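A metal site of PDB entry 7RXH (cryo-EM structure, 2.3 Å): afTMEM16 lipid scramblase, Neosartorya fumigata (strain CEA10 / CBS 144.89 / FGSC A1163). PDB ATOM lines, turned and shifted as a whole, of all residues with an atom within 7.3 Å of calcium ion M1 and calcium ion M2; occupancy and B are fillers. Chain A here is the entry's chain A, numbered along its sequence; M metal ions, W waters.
The side-chain carboxylate (OE2) of Glu 543 sits close to the side-chain amide nitrogen (ND2) of Asn 539, 3.2 Å away.
NZ of Lys 550 lies close to OE2 of Glu 445.
NZ of Lys 550 is in salt-bridge range of OD2 of Asp 511 (3.4 Å).
OH of Tyr 506 sits at hydrogen-bond distance from OD2 of Asp 511 (2.5 Å).
The side-chain carboxylate (OD1) of Asp 547 lies close to the side-chain amino group (NZ) of Lys 550 (3.4 Å).
Lys 550 touches calcium ion M2.
Six residues have an atom within 4 Å of calcium ion M2: Glu 445, Asp 511, Glu 514, Glu 543, Asp 547 and Lys 550.
Calcium ion M1 is bound by OE2 of Glu 514 (2.4 Å), water W2 (2.5 Å), OE1 of Glu 445 (2.6 Å), OE2 of Glu 543 (2.7 Å) and OE1 of Glu 543 (2.7 Å).
OE1 of Glu 543 is bound to calcium ion M2, at 2.4 Å.
Calcium ion M2 is bound by OE2 of Glu 445 (2.4 Å).
OD1 of Asp 511 binds calcium ion M2.
Water W1 binds calcium ion M2 (2.6 Å).
The side-chain carboxylate (OE1) of Glu 514 binds calcium ion M2 (2.6 Å).
OD1 of Asp 547 is bound to calcium ion M2.
Calcium ion M2 is bound by OD2 of Asp 547, at 2.7 Å.
Water W2 bridges the side-chain amide oxygen (OD1) of Asn 539 (2.6 Å) and the backbone carbonyl oxygen (O) of Gln 438 (3.0 Å).
Water W1 lies within hydrogen-bond range of OH of Tyr 180 (2.9 Å) and O of Asp 511 (3.0 Å).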
ATOM      1  N   TYR A 180      -1.309  29.434  32.803  1.00  0.00           N
ATOM      2  CA  TYR A 180      -1.655  29.089  31.433  1.00  0.00           C
ATOM      3  C   TYR A 180      -1.327  27.644  31.127  1.00  0.00           C
ATOM      4  O   TYR A 180      -2.142  26.923  30.540  1.00  0.00           O
ATOM      5  CB  TYR A 180      -0.961  29.999  30.431  1.00  0.00           C
ATOM      6  CG  TYR A 180      -0.969  29.388  29.036  1.00  0.00           C
ATOM      7  CD1 TYR A 180      -2.157  29.232  28.335  1.00  0.00           C
ATOM      8  CD2 TYR A 180       0.203  28.951  28.440  1.00  0.00           C
ATOM      9  CE1 TYR A 180      -2.170  28.675  27.083  1.00  0.00           C
ATOM     10  CE2 TYR A 180       0.190  28.393  27.188  1.00  0.00           C
ATOM     11  CZ  TYR A 180      -1.000  28.253  26.512  1.00  0.00           C
ATOM     12  OH  TYR A 180      -1.013  27.695  25.260  1.00  0.00           O
ATOM     13  N   LEU A 184      -3.900  24.655  30.219  1.00  0.00           N
ATOM     14  CA  LEU A 184      -3.779  23.898  28.975  1.00  0.00           C
ATOM     15  C   LEU A 184      -3.683  22.407  29.244  1.00  0.00           C
ATOM     16  O   LEU A 184      -4.303  21.599  28.553  1.00  0.00           O
ATOM     17  CB  LEU A 184      -2.569  24.375  28.182  1.00  0.00           C
ATOM     18  CG  LEU A 184      -2.355  23.750  26.808  1.00  0.00           C
ATOM     19  CD1 LEU A 184      -3.618  23.806  25.977  1.00  0.00           C
ATOM     20  CD2 LEU A 184      -1.219  24.415  26.075  1.00  0.00           C
ATOM     21  N   ALA A 437      -7.184  25.476  10.201  1.00  0.00           N
ATOM     22  CA  ALA A 437      -6.788  26.654  10.947  1.00  0.00           C
ATOM     23  C   ALA A 437      -5.829  26.314  12.079  1.00  0.00           C
ATOM     24  O   ALA A 437      -4.899  27.067  12.344  1.00  0.00           O
ATOM     25  CB  ALA A 437      -8.015  27.383  11.490  1.00  0.00           C
ATOM     26  N   GLN A 438      -6.015  25.152  12.729  1.00  0.00           N
ATOM     27  CA  GLN A 438      -5.091  24.748  13.780  1.00  0.00           C
ATOM     28  C   GLN A 438      -3.690  24.519  13.230  1.00  0.00           C
ATOM     29  O   GLN A 438      -2.699  24.989  13.798  1.00  0.00           O
ATOM     30  CB  GLN A 438      -5.589  23.476  14.467  1.00  0.00           C
ATOM     31  CG  GLN A 438      -7.036  23.520  14.901  1.00  0.00           C
ATOM     32  CD  GLN A 438      -7.292  24.519  16.009  1.00  0.00           C
ATOM     33  OE1 GLN A 438      -8.012  25.495  15.824  1.00  0.00           O
ATOM     34  NE2 GLN A 438      -6.703  24.271  17.168  1.00  0.00           N
ATOM     35  N   ILE A 439      -3.585  23.793  12.103  1.00  0.00           N
ATOM     36  CA  ILE A 439      -2.277  23.518  11.522  1.00  0.00           C
ATOM     37  C   ILE A 439      -1.625  24.805  11.018  1.00  0.00           C
ATOM     38  O   ILE A 439      -0.429  25.053  11.268  1.00  0.00           O
ATOM     39  CB  ILE A 439      -2.396  22.472  10.402  1.00  0.00           C
ATOM     40  CG1 ILE A 439      -2.943  21.162  10.965  1.00  0.00           C
ATOM     41  CG2 ILE A 439      -1.061  22.240   9.736  1.00  0.00           C
ATOM     42  CD1 ILE A 439      -3.489  20.225   9.922  1.00  0.00           C
ATOM     43  N   VAL A 440      -2.381  25.652  10.323  1.00  0.00           N
ATOM     44  CA  VAL A 440      -1.821  26.892   9.788  1.00  0.00           C
ATOM     45  C   VAL A 440      -1.440  27.832  10.921  1.00  0.00           C
ATOM     46  O   VAL A 440      -0.467  28.583  10.815  1.00  0.00           O
ATOM     47  CB  VAL A 440      -2.820  27.536   8.816  1.00  0.00           C
ATOM     48  CG1 VAL A 440      -2.336  28.906   8.392  1.00  0.00           C
ATOM     49  CG2 VAL A 440      -3.039  26.644   7.612  1.00  0.00           C
ATOM     50  N   GLY A 441      -2.193  27.822  12.014  1.00  0.00           N
ATOM     51  CA  GLY A 441      -1.855  28.650  13.151  1.00  0.00           C
ATOM     52  C   GLY A 441      -0.631  28.162  13.872  1.00  0.00           C
ATOM     53  O   GLY A 441       0.178  28.958  14.332  1.00  0.00           O
ATOM     54  N   PHE A 442      -0.473  26.839  13.991  1.00  0.00           N
ATOM     55  CA  PHE A 442       0.781  26.294  14.494  1.00  0.00           C
ATOM     56  C   PHE A 442       1.951  26.763  13.656  1.00  0.00           C
ATOM     57  O   PHE A 442       2.986  27.193  14.192  1.00  0.00           O
ATOM     58  CB  PHE A 442       0.713  24.763  14.524  1.00  0.00           C
ATOM     59  CG  PHE A 442       2.059  24.100  14.671  1.00  0.00           C
ATOM     60  CD1 PHE A 442       2.655  23.994  15.908  1.00  0.00           C
ATOM     61  CD2 PHE A 442       2.708  23.577  13.569  1.00  0.00           C
ATOM     62  CE1 PHE A 442       3.886  23.380  16.054  1.00  0.00           C
ATOM     63  CE2 PHE A 442       3.938  22.965  13.701  1.00  0.00           C
ATOM     64  CZ  PHE A 442       4.524  22.864  14.947  1.00  0.00           C
ATOM     65  N   ALA A 443       1.808  26.706  12.329  1.00  0.00           N
ATOM     66  CA  ALA A 443       2.860  27.188  11.445  1.00  0.00           C
ATOM     67  C   ALA A 443       3.169  28.661  11.696  1.00  0.00           C
ATOM     68  O   ALA A 443       4.288  29.018  12.090  1.00  0.00           O
ATOM     69  CB  ALA A 443       2.472  26.958   9.987  1.00  0.00           C
ATOM     70  N   GLU A 445       2.571  30.499  14.121  1.00  0.00           N
ATOM     71  CA  GLU A 445       2.891  30.829  15.502  1.00  0.00           C
ATOM     72  C   GLU A 445       4.288  30.399  15.901  1.00  0.00           C
ATOM     73  O   GLU A 445       4.990  31.147  16.583  1.00  0.00           O
ATOM     74  CB  GLU A 445       1.863  30.177  16.433  1.00  0.00           C
ATOM     75  CG  GLU A 445       2.002  30.552  17.887  1.00  0.00           C
ATOM     76  CD  GLU A 445       0.888  29.971  18.734  1.00  0.00           C
ATOM     77  OE1 GLU A 445       0.105  29.145  18.216  1.00  0.00           O
ATOM     78  OE2 GLU A 445       0.786  30.345  19.915  1.00  0.00           O
ATOM     79  N   THR A 446       4.715  29.206  15.493  1.00  0.00           N
ATOM     80  CA  THR A 446       6.048  28.719  15.864  1.00  0.00           C
ATOM     81  C   THR A 446       7.048  28.774  14.734  1.00  0.00           C
ATOM     82  O   THR A 446       8.172  29.224  14.946  1.00  0.00           O
ATOM     83  CB  THR A 446       5.963  27.285  16.389  1.00  0.00           C
ATOM     84  OG1 THR A 446       5.482  26.409  15.360  1.00  0.00           O
ATOM     85  CG2 THR A 446       5.045  27.203  17.599  1.00  0.00           C
ATOM     86  N   TYR A 506       6.832  37.939  25.010  1.00  0.00           N
ATOM     87  CA  TYR A 506       5.773  36.952  25.177  1.00  0.00           C
ATOM     88  C   TYR A 506       4.618  37.536  25.990  1.00  0.00           C
ATOM     89  O   TYR A 506       4.830  38.121  27.049  1.00  0.00           O
ATOM     90  CB  TYR A 506       6.301  35.697  25.859  1.00  0.00           C
ATOM     91  CG  TYR A 506       5.240  34.650  26.078  1.00  0.00           C
ATOM     92  CD1 TYR A 506       4.690  33.954  25.013  1.00  0.00           C
ATOM     93  CD2 TYR A 506       4.767  34.375  27.358  1.00  0.00           C
ATOM     94  CE1 TYR A 506       3.711  33.008  25.211  1.00  0.00           C
ATOM     95  CE2 TYR A 506       3.788  33.429  27.556  1.00  0.00           C
ATOM     96  CZ  TYR A 506       3.263  32.748  26.479  1.00  0.00           C
ATOM     97  OH  TYR A 506       2.284  31.802  26.677  1.00  0.00           O
ATOM     98  N   ASP A 510      -2.206  35.998  24.676  1.00  0.00           N
ATOM     99  CA  ASP A 510      -2.435  35.512  23.321  1.00  0.00           C
ATOM    100  C   ASP A 510      -2.706  34.010  23.309  1.00  0.00           C
ATOM    101  O   ASP A 510      -3.626  33.545  22.625  1.00  0.00           O
ATOM    102  CB  ASP A 510      -1.242  35.835  22.433  1.00  0.00           C
ATOM    103  CG  ASP A 510      -0.895  37.304  22.449  1.00  0.00           C
ATOM    104  OD1 ASP A 510      -1.814  38.136  22.517  1.00  0.00           O
ATOM    105  OD2 ASP A 510       0.319  37.622  22.403  1.00  0.00           O
ATOM    106  N   ASP A 511      -1.936  33.242  24.073  1.00  0.00           N
ATOM    107  CA  ASP A 511      -2.132  31.806  24.120  1.00  0.00           C
ATOM    108  C   ASP A 511      -3.443  31.455  24.807  1.00  0.00           C
ATOM    109  O   ASP A 511      -4.161  30.535  24.382  1.00  0.00           O
ATOM    110  CB  ASP A 511      -0.953  31.145  24.815  1.00  0.00           C
ATOM    111  CG  ASP A 511       0.285  31.102  23.934  1.00  0.00           C
ATOM    112  OD1 ASP A 511       0.142  31.267  22.718  1.00  0.00           O
ATOM    113  OD2 ASP A 511       1.394  30.912  24.467  1.00  0.00           O
ATOM    114  N   LEU A 512      -3.781  32.174  25.885  1.00  0.00           N
ATOM    115  CA  LEU A 512      -5.074  31.966  26.533  1.00  0.00           C
ATOM    116  C   LEU A 512      -6.219  32.287  25.582  1.00  0.00           C
ATOM    117  O   LEU A 512      -7.220  31.561  25.534  1.00  0.00           O
ATOM    118  CB  LEU A 512      -5.175  32.794  27.801  1.00  0.00           C
ATOM    119  CG  LEU A 512      -4.405  32.237  29.000  1.00  0.00           C
ATOM    120  CD1 LEU A 512      -4.167  33.330  30.019  1.00  0.00           C
ATOM    121  CD2 LEU A 512      -5.149  31.063  29.605  1.00  0.00           C
ATOM    122  N   GLU A 514      -6.167  32.075  22.310  1.00  0.00           N
ATOM    123  CA  GLU A 514      -6.247  31.004  21.322  1.00  0.00           C
ATOM    124  C   GLU A 514      -6.955  29.779  21.878  1.00  0.00           C
ATOM    125  O   GLU A 514      -7.844  29.217  21.236  1.00  0.00           O
ATOM    126  CB  GLU A 514      -4.851  30.635  20.826  1.00  0.00           C
ATOM    127  CG  GLU A 514      -4.835  29.508  19.830  1.00  0.00           C
ATOM    128  CD  GLU A 514      -3.450  28.984  19.530  1.00  0.00           C
ATOM    129  OE1 GLU A 514      -2.462  29.687  19.834  1.00  0.00           O
ATOM    130  OE2 GLU A 514      -3.347  27.864  18.993  1.00  0.00           O
ATOM    131  N   MET A 515      -6.604  29.372  23.099  1.00  0.00           N
ATOM    132  CA  MET A 515      -7.237  28.197  23.687  1.00  0.00           C
ATOM    133  C   MET A 515      -8.711  28.436  23.965  1.00  0.00           C
ATOM    134  O   MET A 515      -9.541  27.528  23.784  1.00  0.00           O
ATOM    135  CB  MET A 515      -6.509  27.773  24.955  1.00  0.00           C
ATOM    136  CG  MET A 515      -5.182  27.080  24.681  1.00  0.00           C
ATOM    137  SD  MET A 515      -5.330  25.634  23.613  1.00  0.00           S
ATOM    138  CE  MET A 515      -4.811  26.320  22.037  1.00  0.00           C
ATOM    139  N   GLN A 518     -10.630  28.275  20.702  1.00  0.00           N
ATOM    140  CA  GLN A 518     -10.758  26.874  20.319  1.00  0.00           C
ATOM    141  C   GLN A 518     -11.865  26.185  21.112  1.00  0.00           C
ATOM    142  O   GLN A 518     -12.699  25.446  20.557  1.00  0.00           O
ATOM    143  CB  GLN A 518      -9.415  26.167  20.543  1.00  0.00           C
ATOM    144  CG  GLN A 518      -9.364  24.757  20.032  1.00  0.00           C
ATOM    145  CD  GLN A 518      -8.319  23.941  20.737  1.00  0.00           C
ATOM    146  OE1 GLN A 518      -8.538  23.446  21.829  1.00  0.00           O
ATOM    147  NE2 GLN A 518      -7.166  23.796  20.109  1.00  0.00           N
ATOM    148  N   ASN A 539      -4.082  18.655  18.820  1.00  0.00           N
ATOM    149  CA  ASN A 539      -3.492  19.983  18.726  1.00  0.00           C
ATOM    150  C   ASN A 539      -3.036  20.484  20.081  1.00  0.00           C
ATOM    151  O   ASN A 539      -2.026  21.183  20.165  1.00  0.00           O
ATOM    152  CB  ASN A 539      -4.482  20.970  18.120  1.00  0.00           C
ATOM    153  CG  ASN A 539      -3.936  22.385  18.091  1.00  0.00           C
ATOM    154  OD1 ASN A 539      -3.233  22.770  17.168  1.00  0.00           O
ATOM    155  ND2 ASN A 539      -4.255  23.159  19.117  1.00  0.00           N
ATOM    156  N   VAL A 542       0.174  18.921  21.219  1.00  0.00           N
ATOM    157  CA  VAL A 542       1.269  19.600  20.533  1.00  0.00           C
ATOM    158  C   VAL A 542       1.409  21.038  21.019  1.00  0.00           C
ATOM    159  O   VAL A 542       2.511  21.601  21.004  1.00  0.00           O
ATOM    160  CB  VAL A 542       1.064  19.529  19.008  1.00  0.00           C
ATOM    161  CG1 VAL A 542       1.985  20.512  18.318  1.00  0.00           C
ATOM    162  CG2 VAL A 542       1.305  18.126  18.503  1.00  0.00           C
ATOM    163  N   GLU A 543       0.313  21.646  21.480  1.00  0.00           N
ATOM    164  CA  GLU A 543       0.306  23.060  21.831  1.00  0.00           C
ATOM    165  C   GLU A 543       1.101  23.325  23.088  1.00  0.00           C
ATOM    166  O   GLU A 543       1.802  24.331  23.177  1.00  0.00           O
ATOM    167  CB  GLU A 543      -1.138  23.531  22.003  1.00  0.00           C
ATOM    168  CG  GLU A 543      -1.296  25.036  22.110  1.00  0.00           C
ATOM    169  CD  GLU A 543      -1.285  25.702  20.756  1.00  0.00           C
ATOM    170  OE1 GLU A 543      -0.816  26.848  20.665  1.00  0.00           O
ATOM    171  OE2 GLU A 543      -1.741  25.072  19.785  1.00  0.00           O
ATOM    172  N   LEU A 544       0.986  22.439  24.085  1.00  0.00           N
ATOM    173  CA  LEU A 544       1.832  22.550  25.283  1.00  0.00           C
ATOM    174  C   LEU A 544       3.303  22.650  24.911  1.00  0.00           C
ATOM    175  O   LEU A 544       3.986  23.628  25.264  1.00  0.00           O
ATOM    176  CB  LEU A 544       1.591  21.353  26.201  1.00  0.00           C
ATOM    177  CG  LEU A 544       0.276  21.311  26.962  1.00  0.00           C
ATOM    178  CD1 LEU A 544       0.042  19.937  27.554  1.00  0.00           C
ATOM    179  CD2 LEU A 544       0.290  22.333  28.070  1.00  0.00           C
ATOM    180  N   SER A 546       4.801  23.111  21.921  1.00  0.00           N
ATOM    181  CA  SER A 546       5.172  24.160  20.980  1.00  0.00           C
ATOM    182  C   SER A 546       5.093  25.538  21.614  1.00  0.00           C
ATOM    183  O   SER A 546       5.902  26.404  21.284  1.00  0.00           O
ATOM    184  CB  SER A 546       4.301  24.082  19.733  1.00  0.00           C
ATOM    185  OG  SER A 546       3.086  24.775  19.896  1.00  0.00           O
ATOM    186  N   ASP A 547       4.180  25.763  22.555  1.00  0.00           N
ATOM    187  CA  ASP A 547       4.143  27.030  23.265  1.00  0.00           C
ATOM    188  C   ASP A 547       5.318  27.165  24.208  1.00  0.00           C
ATOM    189  O   ASP A 547       5.902  28.254  24.334  1.00  0.00           O
ATOM    190  CB  ASP A 547       2.822  27.176  24.026  1.00  0.00           C
ATOM    191  CG  ASP A 547       1.709  27.706  23.161  1.00  0.00           C
ATOM    192  OD1 ASP A 547       2.004  28.254  22.087  1.00  0.00           O
ATOM    193  OD2 ASP A 547       0.534  27.580  23.557  1.00  0.00           O
ATOM    194  N   LYS A 550       8.160  28.064  21.990  1.00  0.00           N
ATOM    195  CA  LYS A 550       8.068  29.453  21.588  1.00  0.00           C
ATOM    196  C   LYS A 550       8.524  30.388  22.697  1.00  0.00           C
ATOM    197  O   LYS A 550       9.229  31.368  22.439  1.00  0.00           O
ATOM    198  CB  LYS A 550       6.632  29.779  21.173  1.00  0.00           C
ATOM    199  CG  LYS A 550       6.376  31.235  20.877  1.00  0.00           C
ATOM    200  CD  LYS A 550       4.936  31.460  20.497  1.00  0.00           C
ATOM    201  CE  LYS A 550       4.010  31.245  21.682  1.00  0.00           C
ATOM    202  NZ  LYS A 550       2.601  31.498  21.337  1.00  0.00           N
HETATM  203 CA    CA M   1      -1.319  27.026  18.018  1.00  0.00          CA
HETATM  204 CA    CA M   2      -0.498  29.075  21.495  1.00  0.00          CA
HETATM  205  O   HOH W   1      -2.567  28.436  22.976  1.00  0.00           O
HETATM  206  O   HOH W   2      -2.561  25.217  16.765  1.00  0.00           O
